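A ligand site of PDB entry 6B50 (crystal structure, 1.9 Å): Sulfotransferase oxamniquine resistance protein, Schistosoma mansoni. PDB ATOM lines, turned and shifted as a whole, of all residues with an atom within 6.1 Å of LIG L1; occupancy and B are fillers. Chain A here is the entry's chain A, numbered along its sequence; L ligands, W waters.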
ATOM      1  N   LEU A  17       2.671 -10.413  11.488  1.00  0.00           N
ATOM      2  CA  LEU A  17       1.957 -10.852  12.694  1.00  0.00           C
ATOM      3  C   LEU A  17       2.633 -12.025  13.395  1.00  0.00           C
ATOM      4  O   LEU A  17       3.442 -12.733  12.776  1.00  0.00           O
ATOM      5  CB  LEU A  17       0.522 -11.242  12.327  1.00  0.00           C
ATOM      6  CG  LEU A  17      -0.337 -10.121  11.730  1.00  0.00           C
ATOM      7  CD1 LEU A  17      -1.607 -10.688  11.136  1.00  0.00           C
ATOM      8  CD2 LEU A  17      -0.629  -9.073  12.756  1.00  0.00           C
ATOM      9  N   PRO A  18       2.307 -12.250  14.671  1.00  0.00           N
ATOM     10  CA  PRO A  18       2.868 -13.432  15.330  1.00  0.00           C
ATOM     11  C   PRO A  18       2.563 -14.729  14.561  1.00  0.00           C
ATOM     12  O   PRO A  18       1.536 -14.801  13.869  1.00  0.00           O
ATOM     13  CB  PRO A  18       2.168 -13.444  16.711  1.00  0.00           C
ATOM     14  CG  PRO A  18       1.180 -12.346  16.690  1.00  0.00           C
ATOM     15  CD  PRO A  18       1.547 -11.396  15.610  1.00  0.00           C
ATOM     16  N   ARG A  19       3.485 -15.692  14.655  1.00  0.00           N
ATOM     17  CA  ARG A  19       3.391 -17.007  14.020  1.00  0.00           C
ATOM     18  C   ARG A  19       3.613 -16.943  12.514  1.00  0.00           C
ATOM     19  O   ARG A  19       3.095 -17.787  11.777  1.00  0.00           O
ATOM     20  CB  ARG A  19       2.040 -17.708  14.327  1.00  0.00           C
ATOM     21  CG  ARG A  19       1.667 -17.786  15.812  1.00  0.00           C
ATOM     22  CD  ARG A  19       2.843 -18.220  16.691  1.00  0.00           C
ATOM     23  NE  ARG A  19       3.254 -19.597  16.422  1.00  0.00           N
ATOM     24  CZ  ARG A  19       4.340 -20.167  16.927  1.00  0.00           C
ATOM     25  NH1 ARG A  19       5.146 -19.456  17.722  1.00  0.00           N
ATOM     26  NH2 ARG A  19       4.636 -21.421  16.631  1.00  0.00           N
ATOM     27  N   THR A  20       4.384 -15.949  12.055  1.00  0.00           N
ATOM     28  CA  THR A  20       4.747 -15.834  10.642  1.00  0.00           C
ATOM     29  C   THR A  20       6.256 -15.882  10.428  1.00  0.00           C
ATOM     30  O   THR A  20       6.762 -15.431   9.399  1.00  0.00           O
ATOM     31  CB  THR A  20       4.197 -14.533  10.010  1.00  0.00           C
ATOM     32  OG1 THR A  20       4.745 -13.402  10.687  1.00  0.00           O
ATOM     33  CG2 THR A  20       2.684 -14.500  10.106  1.00  0.00           C
ATOM     34  N   GLY A  21       6.976 -16.470  11.368  1.00  0.00           N
ATOM     35  CA  GLY A  21       8.430 -16.527  11.276  1.00  0.00           C
ATOM     36  C   GLY A  21       9.142 -15.328  11.898  1.00  0.00           C
ATOM     37  O   GLY A  21      10.277 -15.009  11.519  1.00  0.00           O
ATOM     38  N   THR A  22       8.497 -14.675  12.873  1.00  0.00           N
ATOM     39  CA  THR A  22       9.063 -13.425  13.426  1.00  0.00           C
ATOM     40  C   THR A  22      10.284 -13.704  14.296  1.00  0.00           C
ATOM     41  O   THR A  22      11.223 -12.938  14.301  1.00  0.00           O
ATOM     42  CB  THR A  22       8.044 -12.620  14.246  1.00  0.00           C
ATOM     43  OG1 THR A  22       7.593 -13.398  15.371  1.00  0.00           O
ATOM     44  CG2 THR A  22       6.848 -12.242  13.407  1.00  0.00           C
ATOM     45  N   LYS A  23      10.292 -14.826  15.025  1.00  0.00           N
ATOM     46  CA  LYS A  23      11.454 -15.104  15.871  1.00  0.00           C
ATOM     47  C   LYS A  23      12.661 -15.505  15.011  1.00  0.00           C
ATOM     48  O   LYS A  23      13.782 -15.123  15.306  1.00  0.00           O
ATOM     49  CB  LYS A  23      11.141 -16.198  16.894  1.00  0.00           C
ATOM     50  CG  LYS A  23      12.312 -16.535  17.837  1.00  0.00           C
ATOM     51  CD  LYS A  23      12.694 -15.304  18.659  1.00  0.00           C
ATOM     52  CE  LYS A  23      13.589 -15.644  19.853  1.00  0.00           C
ATOM     53  NZ  LYS A  23      14.936 -16.140  19.502  1.00  0.00           N
ATOM     54  N   SER A  24      12.434 -16.269  13.941  1.00  0.00           N
ATOM     55  CA  SER A  24      13.527 -16.554  13.020  1.00  0.00           C
ATOM     56  C   SER A  24      14.090 -15.266  12.410  1.00  0.00           C
ATOM     57  O   SER A  24      15.299 -15.131  12.249  1.00  0.00           O
ATOM     58  CB  SER A  24      13.081 -17.507  11.921  1.00  0.00           C
ATOM     59  OG  SER A  24      12.783 -18.772  12.479  1.00  0.00           O
ATOM     60  N   HIS A  39      11.178  -8.032  19.879  1.00  0.00           N
ATOM     61  CA  HIS A  39      10.290  -9.173  19.661  1.00  0.00           C
ATOM     62  C   HIS A  39       9.527  -9.381  20.962  1.00  0.00           C
ATOM     63  O   HIS A  39       9.970  -8.919  22.000  1.00  0.00           O
ATOM     64  CB  HIS A  39      11.080 -10.438  19.284  1.00  0.00           C
ATOM     65  CG  HIS A  39      10.232 -11.593  18.843  1.00  0.00           C
ATOM     66  ND1 HIS A  39       9.663 -12.483  19.735  1.00  0.00           N
ATOM     67  CD2 HIS A  39       9.881 -12.022  17.607  1.00  0.00           C
ATOM     68  CE1 HIS A  39       8.987 -13.392  19.065  1.00  0.00           C
ATOM     69  NE2 HIS A  39       9.101 -13.148  17.770  1.00  0.00           N
ATOM     70  N   ASP A  93       7.179  -8.557  15.471  1.00  0.00           N
ATOM     71  CA  ASP A  93       6.174  -9.174  16.333  1.00  0.00           C
ATOM     72  C   ASP A  93       5.317  -8.159  17.103  1.00  0.00           C
ATOM     73  O   ASP A  93       5.584  -6.957  17.083  1.00  0.00           O
ATOM     74  CB  ASP A  93       6.882 -10.112  17.320  1.00  0.00           C
ATOM     75  CG  ASP A  93       5.961 -11.113  17.969  1.00  0.00           C
ATOM     76  OD1 ASP A  93       4.794 -11.258  17.534  1.00  0.00           O
ATOM     77  OD2 ASP A  93       6.420 -11.768  18.919  1.00  0.00           O
ATOM     78  N   ARG A 117       2.247 -16.014   5.566  1.00  0.00           N
ATOM     79  CA  ARG A 117       2.160 -17.450   5.329  1.00  0.00           C
ATOM     80  C   ARG A 117       0.714 -17.849   5.068  1.00  0.00           C
ATOM     81  O   ARG A 117      -0.204 -17.029   5.198  1.00  0.00           O
ATOM     82  CB  ARG A 117       2.702 -18.236   6.523  1.00  0.00           C
ATOM     83  CG  ARG A 117       1.750 -18.269   7.703  1.00  0.00           C
ATOM     84  CD  ARG A 117       2.409 -18.869   8.958  1.00  0.00           C
ATOM     85  NE  ARG A 117       2.563 -20.320   8.871  1.00  0.00           N
ATOM     86  CZ  ARG A 117       2.868 -21.103   9.899  1.00  0.00           C
ATOM     87  NH1 ARG A 117       3.058 -20.570  11.112  1.00  0.00           N
ATOM     88  NH2 ARG A 117       2.978 -22.425   9.744  1.00  0.00           N
ATOM     89  N   ASP A 121      -2.544 -22.322   8.136  1.00  0.00           N
ATOM     90  CA  ASP A 121      -1.363 -22.695   8.918  1.00  0.00           C
ATOM     91  C   ASP A 121      -1.113 -21.670  10.036  1.00  0.00           C
ATOM     92  O   ASP A 121      -0.747 -22.037  11.141  1.00  0.00           O
ATOM     93  CB  ASP A 121      -0.103 -22.787   8.062  1.00  0.00           C
ATOM     94  CG  ASP A 121      -0.090 -24.015   7.153  1.00  0.00           C
ATOM     95  OD1 ASP A 121      -0.905 -24.934   7.341  1.00  0.00           O
ATOM     96  OD2 ASP A 121       0.765 -24.048   6.246  1.00  0.00           O
ATOM     97  N   SER A 125      -1.274 -22.505  14.064  1.00  0.00           N
ATOM     98  CA  SER A 125      -0.108 -22.165  14.885  1.00  0.00           C
ATOM     99  C   SER A 125      -0.500 -21.204  16.034  1.00  0.00           C
ATOM    100  O   SER A 125      -0.071 -21.377  17.171  1.00  0.00           O
ATOM    101  CB  SER A 125       0.977 -21.521  14.006  1.00  0.00           C
ATOM    102  OG  SER A 125       2.199 -21.358  14.719  1.00  0.00           O
ATOM    103  N   VAL A 129      -0.379 -21.802  20.424  1.00  0.00           N
ATOM    104  CA  VAL A 129       0.709 -21.108  21.100  1.00  0.00           C
ATOM    105  C   VAL A 129       0.278 -19.806  21.765  1.00  0.00           C
ATOM    106  O   VAL A 129       0.575 -19.581  22.941  1.00  0.00           O
ATOM    107  CB  VAL A 129       1.847 -20.816  20.092  1.00  0.00           C
ATOM    108  CG1 VAL A 129       2.818 -19.783  20.639  1.00  0.00           C
ATOM    109  CG2 VAL A 129       2.582 -22.093  19.764  1.00  0.00           C
ATOM    110  N   LEU A 205       7.270 -17.474   4.538  1.00  0.00           N
ATOM    111  CA  LEU A 205       7.972 -18.447   5.347  1.00  0.00           C
ATOM    112  C   LEU A 205       8.787 -19.366   4.457  1.00  0.00           C
ATOM    113  O   LEU A 205       8.256 -19.879   3.478  1.00  0.00           O
ATOM    114  CB  LEU A 205       6.995 -19.298   6.176  1.00  0.00           C
ATOM    115  CG  LEU A 205       6.699 -18.859   7.602  1.00  0.00           C
ATOM    116  CD1 LEU A 205       5.873 -19.938   8.306  1.00  0.00           C
ATOM    117  CD2 LEU A 205       8.005 -18.551   8.337  1.00  0.00           C
ATOM    118  N   GLY A 206      10.061 -19.557   4.788  1.00  0.00           N
ATOM    119  CA  GLY A 206      10.903 -20.439   4.015  1.00  0.00           C
ATOM    120  C   GLY A 206      11.739 -19.773   2.940  1.00  0.00           C
ATOM    121  O   GLY A 206      12.585 -20.429   2.315  1.00  0.00           O
ATOM    122  N   TYR A 226      19.751 -20.028   7.532  1.00  0.00           N
ATOM    123  CA  TYR A 226      18.705 -19.106   7.991  1.00  0.00           C
ATOM    124  C   TYR A 226      17.932 -19.757   9.143  1.00  0.00           C
ATOM    125  O   TYR A 226      17.529 -20.926   9.033  1.00  0.00           O
ATOM    126  CB  TYR A 226      17.772 -18.762   6.849  1.00  0.00           C
ATOM    127  CG  TYR A 226      16.769 -17.706   7.240  1.00  0.00           C
ATOM    128  CD1 TYR A 226      15.544 -18.064   7.809  1.00  0.00           C
ATOM    129  CD2 TYR A 226      17.048 -16.366   7.054  1.00  0.00           C
ATOM    130  CE1 TYR A 226      14.635 -17.110   8.168  1.00  0.00           C
ATOM    131  CE2 TYR A 226      16.143 -15.398   7.417  1.00  0.00           C
ATOM    132  CZ  TYR A 226      14.943 -15.768   7.974  1.00  0.00           C
ATOM    133  OH  TYR A 226      14.053 -14.802   8.330  1.00  0.00           O
ATOM    134  N   PRO A 227      17.725 -19.017  10.243  1.00  0.00           N
ATOM    135  CA  PRO A 227      17.127 -19.610  11.450  1.00  0.00           C
ATOM    136  C   PRO A 227      15.781 -20.292  11.209  1.00  0.00           C
ATOM    137  O   PRO A 227      14.967 -19.837  10.390  1.00  0.00           O
ATOM    138  CB  PRO A 227      16.943 -18.399  12.375  1.00  0.00           C
ATOM    139  CG  PRO A 227      17.954 -17.428  11.920  1.00  0.00           C
ATOM    140  CD  PRO A 227      18.042 -17.591  10.445  1.00  0.00           C
ATOM    141  N   CYS A 228      15.572 -21.398  11.907  1.00  0.00           N
ATOM    142  CA  CYS A 228      14.294 -22.081  11.859  1.00  0.00           C
ATOM    143  C   CYS A 228      13.878 -22.426  13.284  1.00  0.00           C
ATOM    144  O   CYS A 228      14.182 -23.509  13.776  1.00  0.00           O
ATOM    145  CB  CYS A 228      14.377 -23.324  10.988  1.00  0.00           C
ATOM    146  SG  CYS A 228      12.781 -24.081  10.753  1.00  0.00           S
ATOM    147  N   VAL A 229      13.205 -21.497  13.953  1.00  0.00           N
ATOM    148  CA  VAL A 229      12.899 -21.654  15.386  1.00  0.00           C
ATOM    149  C   VAL A 229      11.454 -21.284  15.686  1.00  0.00           C
ATOM    150  O   VAL A 229      10.764 -20.693  14.852  1.00  0.00           O
ATOM    151  CB  VAL A 229      13.822 -20.785  16.264  1.00  0.00           C
ATOM    152  CG1 VAL A 229      15.243 -21.303  16.237  1.00  0.00           C
ATOM    153  CG2 VAL A 229      13.761 -19.308  15.827  1.00  0.00           C
ATOM    154  N   ASN A 230      11.009 -21.661  16.887  1.00  0.00           N
ATOM    155  CA  ASN A 230       9.709 -21.249  17.428  1.00  0.00           C
ATOM    156  C   ASN A 230       8.510 -21.966  16.785  1.00  0.00           C
ATOM    157  O   ASN A 230       7.424 -21.391  16.697  1.00  0.00           O
ATOM    158  CB  ASN A 230       9.553 -19.715  17.310  1.00  0.00           C
ATOM    159  CG  ASN A 230       8.549 -19.143  18.286  1.00  0.00           C
ATOM    160  OD1 ASN A 230       8.120 -19.824  19.213  1.00  0.00           O
ATOM    161  ND2 ASN A 230       8.155 -17.890  18.078  1.00  0.00           N
ATOM    162  N   SER A 231       8.693 -23.217  16.361  1.00  0.00           N
ATOM    163  CA  SER A 231       7.601 -24.050  15.905  1.00  0.00           C
ATOM    164  C   SER A 231       6.638 -24.333  17.069  1.00  0.00           C
ATOM    165  O   SER A 231       7.032 -24.298  18.231  1.00  0.00           O
ATOM    166  CB  SER A 231       8.111 -25.368  15.307  1.00  0.00           C
ATOM    167  OG  SER A 231       8.650 -26.226  16.313  1.00  0.00           O
ATOM    168  N   HIS A 232       5.365 -24.566  16.768  1.00  0.00           N
ATOM    169  CA  HIS A 232       4.431 -24.826  17.869  1.00  0.00           C
ATOM    170  C   HIS A 232       4.840 -26.093  18.638  1.00  0.00           C
ATOM    171  O   HIS A 232       4.619 -26.167  19.834  1.00  0.00           O
ATOM    172  CB  HIS A 232       2.976 -24.910  17.367  1.00  0.00           C
ATOM    173  CG  HIS A 232       2.687 -26.106  16.511  1.00  0.00           C
ATOM    174  ND1 HIS A 232       2.387 -27.337  17.031  1.00  0.00           N
ATOM    175  CD2 HIS A 232       2.635 -26.241  15.165  1.00  0.00           C
ATOM    176  CE1 HIS A 232       2.185 -28.191  16.048  1.00  0.00           C
ATOM    177  NE2 HIS A 232       2.329 -27.547  14.899  1.00  0.00           N
ATOM    178  N   HIS A 233       5.436 -27.063  17.945  1.00  0.00           N
ATOM    179  CA  HIS A 233       5.924 -28.276  18.625  1.00  0.00           C
ATOM    180  C   HIS A 233       6.984 -27.918  19.666  1.00  0.00           C
ATOM    181  O   HIS A 233       6.983 -28.447  20.769  1.00  0.00           O
ATOM    182  CB  HIS A 233       6.529 -29.284  17.632  1.00  0.00           C
ATOM    183  CG  HIS A 233       5.545 -29.834  16.639  1.00  0.00           C
ATOM    184  ND1 HIS A 233       4.511 -30.673  16.989  1.00  0.00           N
ATOM    185  CD2 HIS A 233       5.475 -29.692  15.294  1.00  0.00           C
ATOM    186  CE1 HIS A 233       3.833 -31.005  15.905  1.00  0.00           C
ATOM    187  NE2 HIS A 233       4.390 -30.420  14.861  1.00  0.00           N
HETATM  188  P1  LIG L   1       4.488 -23.473  13.208  1.00  0.00           P
HETATM  189  O1  LIG L   1       3.390 -23.719  12.215  1.00  0.00           O
HETATM  190  O2  LIG L   1       3.913 -23.222  14.581  1.00  0.00           O
HETATM  191  O3  LIG L   1       5.490 -24.593  13.299  1.00  0.00           O
HETATM  192  P2  LIG L   1       6.786 -16.732  15.031  1.00  0.00           P
HETATM  193  O4  LIG L   1       6.373 -15.449  14.376  1.00  0.00           O
HETATM  194  O5  LIG L   1       8.211 -16.755  15.481  1.00  0.00           O
HETATM  195  O6  LIG L   1       5.840 -17.131  16.184  1.00  0.00           O
HETATM  196  O7  LIG L   1       6.606 -17.829  13.880  1.00  0.00           O
HETATM  197  C1  LIG L   1       6.798 -19.224  14.179  1.00  0.00           C
HETATM  198  C2  LIG L   1       6.257 -20.049  13.040  1.00  0.00           C
HETATM  199  O8  LIG L   1       7.070 -19.857  11.839  1.00  0.00           O
HETATM  200  C3  LIG L   1       6.301 -21.521  13.330  1.00  0.00           C
HETATM  201  O9  LIG L   1       5.242 -22.161  12.619  1.00  0.00           O
HETATM  202  C4  LIG L   1       7.603 -21.939  12.757  1.00  0.00           C
HETATM  203  O10 LIG L   1       7.647 -23.318  12.453  1.00  0.00           O
HETATM  204  C5  LIG L   1       7.663 -21.126  11.514  1.00  0.00           C
HETATM  205  N1  LIG L   1       8.980 -20.911  11.047  1.00  0.00           N
HETATM  206  C6  LIG L   1       9.925 -20.177  11.638  1.00  0.00           C
HETATM  207  N2  LIG L   1      11.046 -20.187  10.908  1.00  0.00           N
HETATM  208  C7  LIG L   1      10.815 -20.942   9.780  1.00  0.00           C
HETATM  209  C8  LIG L   1      11.613 -21.304   8.652  1.00  0.00           C
HETATM  210  N3  LIG L   1      12.938 -20.871   8.506  1.00  0.00           N
HETATM  211  N4  LIG L   1      11.051 -22.075   7.711  1.00  0.00           N
HETATM  212  C9  LIG L   1       9.789 -22.493   7.821  1.00  0.00           C
HETATM  213  N5  LIG L   1       9.010 -22.179   8.873  1.00  0.00           N
HETATM  214  C10 LIG L   1       9.484 -21.404   9.871  1.00  0.00           C
HETATM  215  C1  LG2 L   2       4.465 -15.095  21.827  1.00  0.00           C
HETATM  216  C2  LG2 L   2       3.649 -14.015  21.486  1.00  0.00           C
HETATM  217  C3  LG2 L   2       2.530 -13.748  22.302  1.00  0.00           C
HETATM  218  C4  LG2 L   2       2.253 -14.521  23.419  1.00  0.00           C
HETATM  219  C5  LG2 L   2       3.070 -15.602  23.735  1.00  0.00           C
HETATM  220  C6  LG2 L   2       4.172 -15.891  22.933  1.00  0.00           C
HETATM  221  C7  LG2 L   2       3.394 -17.717  25.005  1.00  0.00           C
HETATM  222  C8  LG2 L   2       4.127 -18.111  23.723  1.00  0.00           C
HETATM  223  C9  LG2 L   2       5.001 -16.963  23.258  1.00  0.00           C
HETATM  224  C10 LG2 L   2       3.938 -13.208  20.372  1.00  0.00           C
HETATM  225  C11 LG2 L   2       4.317 -17.868  26.226  1.00  0.00           C
HETATM  226  C12 LG2 L   2       5.733 -20.579  26.289  1.00  0.00           C
HETATM  227  C13 LG2 L   2       4.369 -21.066  28.290  1.00  0.00           C
HETATM  228  C14 LG2 L   2       4.953 -19.942  27.439  1.00  0.00           C
HETATM  229  N1  LG2 L   2       2.752 -16.386  24.853  1.00  0.00           N
HETATM  230  N2  LG2 L   2       1.754 -12.709  21.988  1.00  0.00           N
HETATM  231  N3  LG2 L   2       3.861 -19.059  26.963  1.00  0.00           N
HETATM  232  O1  LG2 L   2       1.517 -11.780  22.951  1.00  0.00           O
HETATM  233  O2  LG2 L   2       1.060 -12.646  20.626  1.00  0.00           O
HETATM  234  O3  LG2 L   2       5.060 -13.722  19.631  1.00  0.00           O
HETATM  235  O   HOH W   1       5.441 -16.216  18.832  1.00  0.00           O
HETATM  236  O   HOH W   2      14.691 -20.871   5.924  1.00  0.00           O
HETATM  237  O   HOH W   3       0.657 -24.511  11.760  1.00  0.00           O
HETATM  238  O   HOH W   4      12.543 -23.447   5.648  1.00  0.00           O
HETATM  239  O   HOH W   5       5.723 -25.425  10.160  1.00  0.00           O
HETATM  240  O   HOH W   6       9.795 -25.489  11.746  1.00  0.00           O
HETATM  241  O   HOH W   7      10.226 -18.069  13.890  1.00  0.00           O
HETATM  242  O   HOH W   8       6.851 -24.053   8.532  1.00  0.00           O
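Pro 18 touches LIG L1. Leu 205 touches LIG L1. Gly 206 touches LIG L1. Tyr 226 touches LIG L1 (CD1 to N3, 3.9 Å). Cys 228 touches LIG L1. Val 229 touches LIG L1 (O to C6, 3.4 Å). Ser 231 touches LIG L1 (CB to O3, 3.4 Å). Hydrophobic or aromatic side chains that line LIG L1: Leu 205, Tyr 226 and His 232.
Water W1 lies within hydrogen-bond range of an oxygen (O3) of LG2 L2 (2.6 Å), an oxygen (O6) of LIG L1 (2.8 Å), the side-chain amide nitrogen of Asn 230 (3.3 Å) and the guanidinium group of Arg 19 (3.4 Å). Water W3 bridges an oxygen (O1) of LIG L1 (2.9 Å) and the backbone carbonyl oxygen of Asp 121 (2.9 Å). Water W7 lies within hydrogen-bond range of the backbone carbonyl oxygen of Val 229, the backbone NH of Ser 24, an oxygen (O5) of LIG L1 and the backbone NH of Lys 23. Water W6 lies within hydrogen-bond range of O10 of LIG L1 and SG of Cys 228.
A ring nitrogen (NE2) of His 39 is in hydrogen-bond range of the side-chain hydroxyl (OG1) of Thr 22, at 2.8 Å. The backbone NH (N) of Lys 23 lies within hydrogen-bond range of a ring nitrogen (NE2) of His 39, at 3.4 Å. The backbone carbonyl oxygen (O) of Leu 17 sits at hydrogen-bond distance from the side-chain hydroxyl (OG1) of Thr 20 (2.6 Å). The side-chain hydroxyl (OG) of Ser 24 is in hydrogen-bond range of the backbone NH (N) of Val 229 (3.1 Å). The side-chain hydroxyl of Ser 24 is in hydrogen-bond range of the backbone carbonyl oxygen of Pro 227, 3.2 Å away. The side-chain hydroxyl (OG) of Ser 125 lies within hydrogen-bond range of the guanidinium group (NE) of Arg 19. The guanidinium group (NH2) of Arg 19 lies within hydrogen-bond range of the backbone carbonyl oxygen (O) of Asn 230 (2.8 Å). O of Arg 19 sits at hydrogen-bond distance from NH1 of Arg 117 (2.9 Å).
OD2 of Asp 93 is in hydrogen-bond range of O3 of LG2 L2, at 2.5 Å. ND2 of Asn 230 is in hydrogen-bond range of O5 of LIG L1 (2.8 Å). An oxygen (O4) of LIG L1 lies within hydrogen-bond range of the backbone NH (N) of Thr 22, at 2.7 Å. The guanidinium group (NH2) of Arg 19 lies within salt-bridge range of an oxygen (O2) of LIG L1 (2.8 Å). O4 of LIG L1 sits at hydrogen-bond distance from N of Thr 20 (3.1 Å). OG of Ser 24 is in hydrogen-bond range of N2 of LIG L1 (2.7 Å). N of Gly 21 is in hydrogen-bond range of O7 of LIG L1 (2.9 Å). The backbone carbonyl oxygen (O) of Pro 227 is in hydrogen-bond range of a nitrogen (N3) of LIG L1, at 3.0 Å. N of His 232 lies within hydrogen-bond range of O2 of LIG L1 (2.9 Å). O5 of LIG L1 sits at hydrogen-bond distance from N of Lys 23, 2.9 Å away. O1 of LIG L1 is in salt-bridge range of NH2 of Arg 117, at 2.8 Å. The side-chain hydroxyl of Thr 22 sits at hydrogen-bond distance from an oxygen (O4) of LIG L1 (2.6 Å). O4 of LIG L1 is in hydrogen-bond range of N of Arg 19. An oxygen (O2) of LIG L1 lies within hydrogen-bond range of the side-chain hydroxyl (OG) of Ser 125 (2.5 Å).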
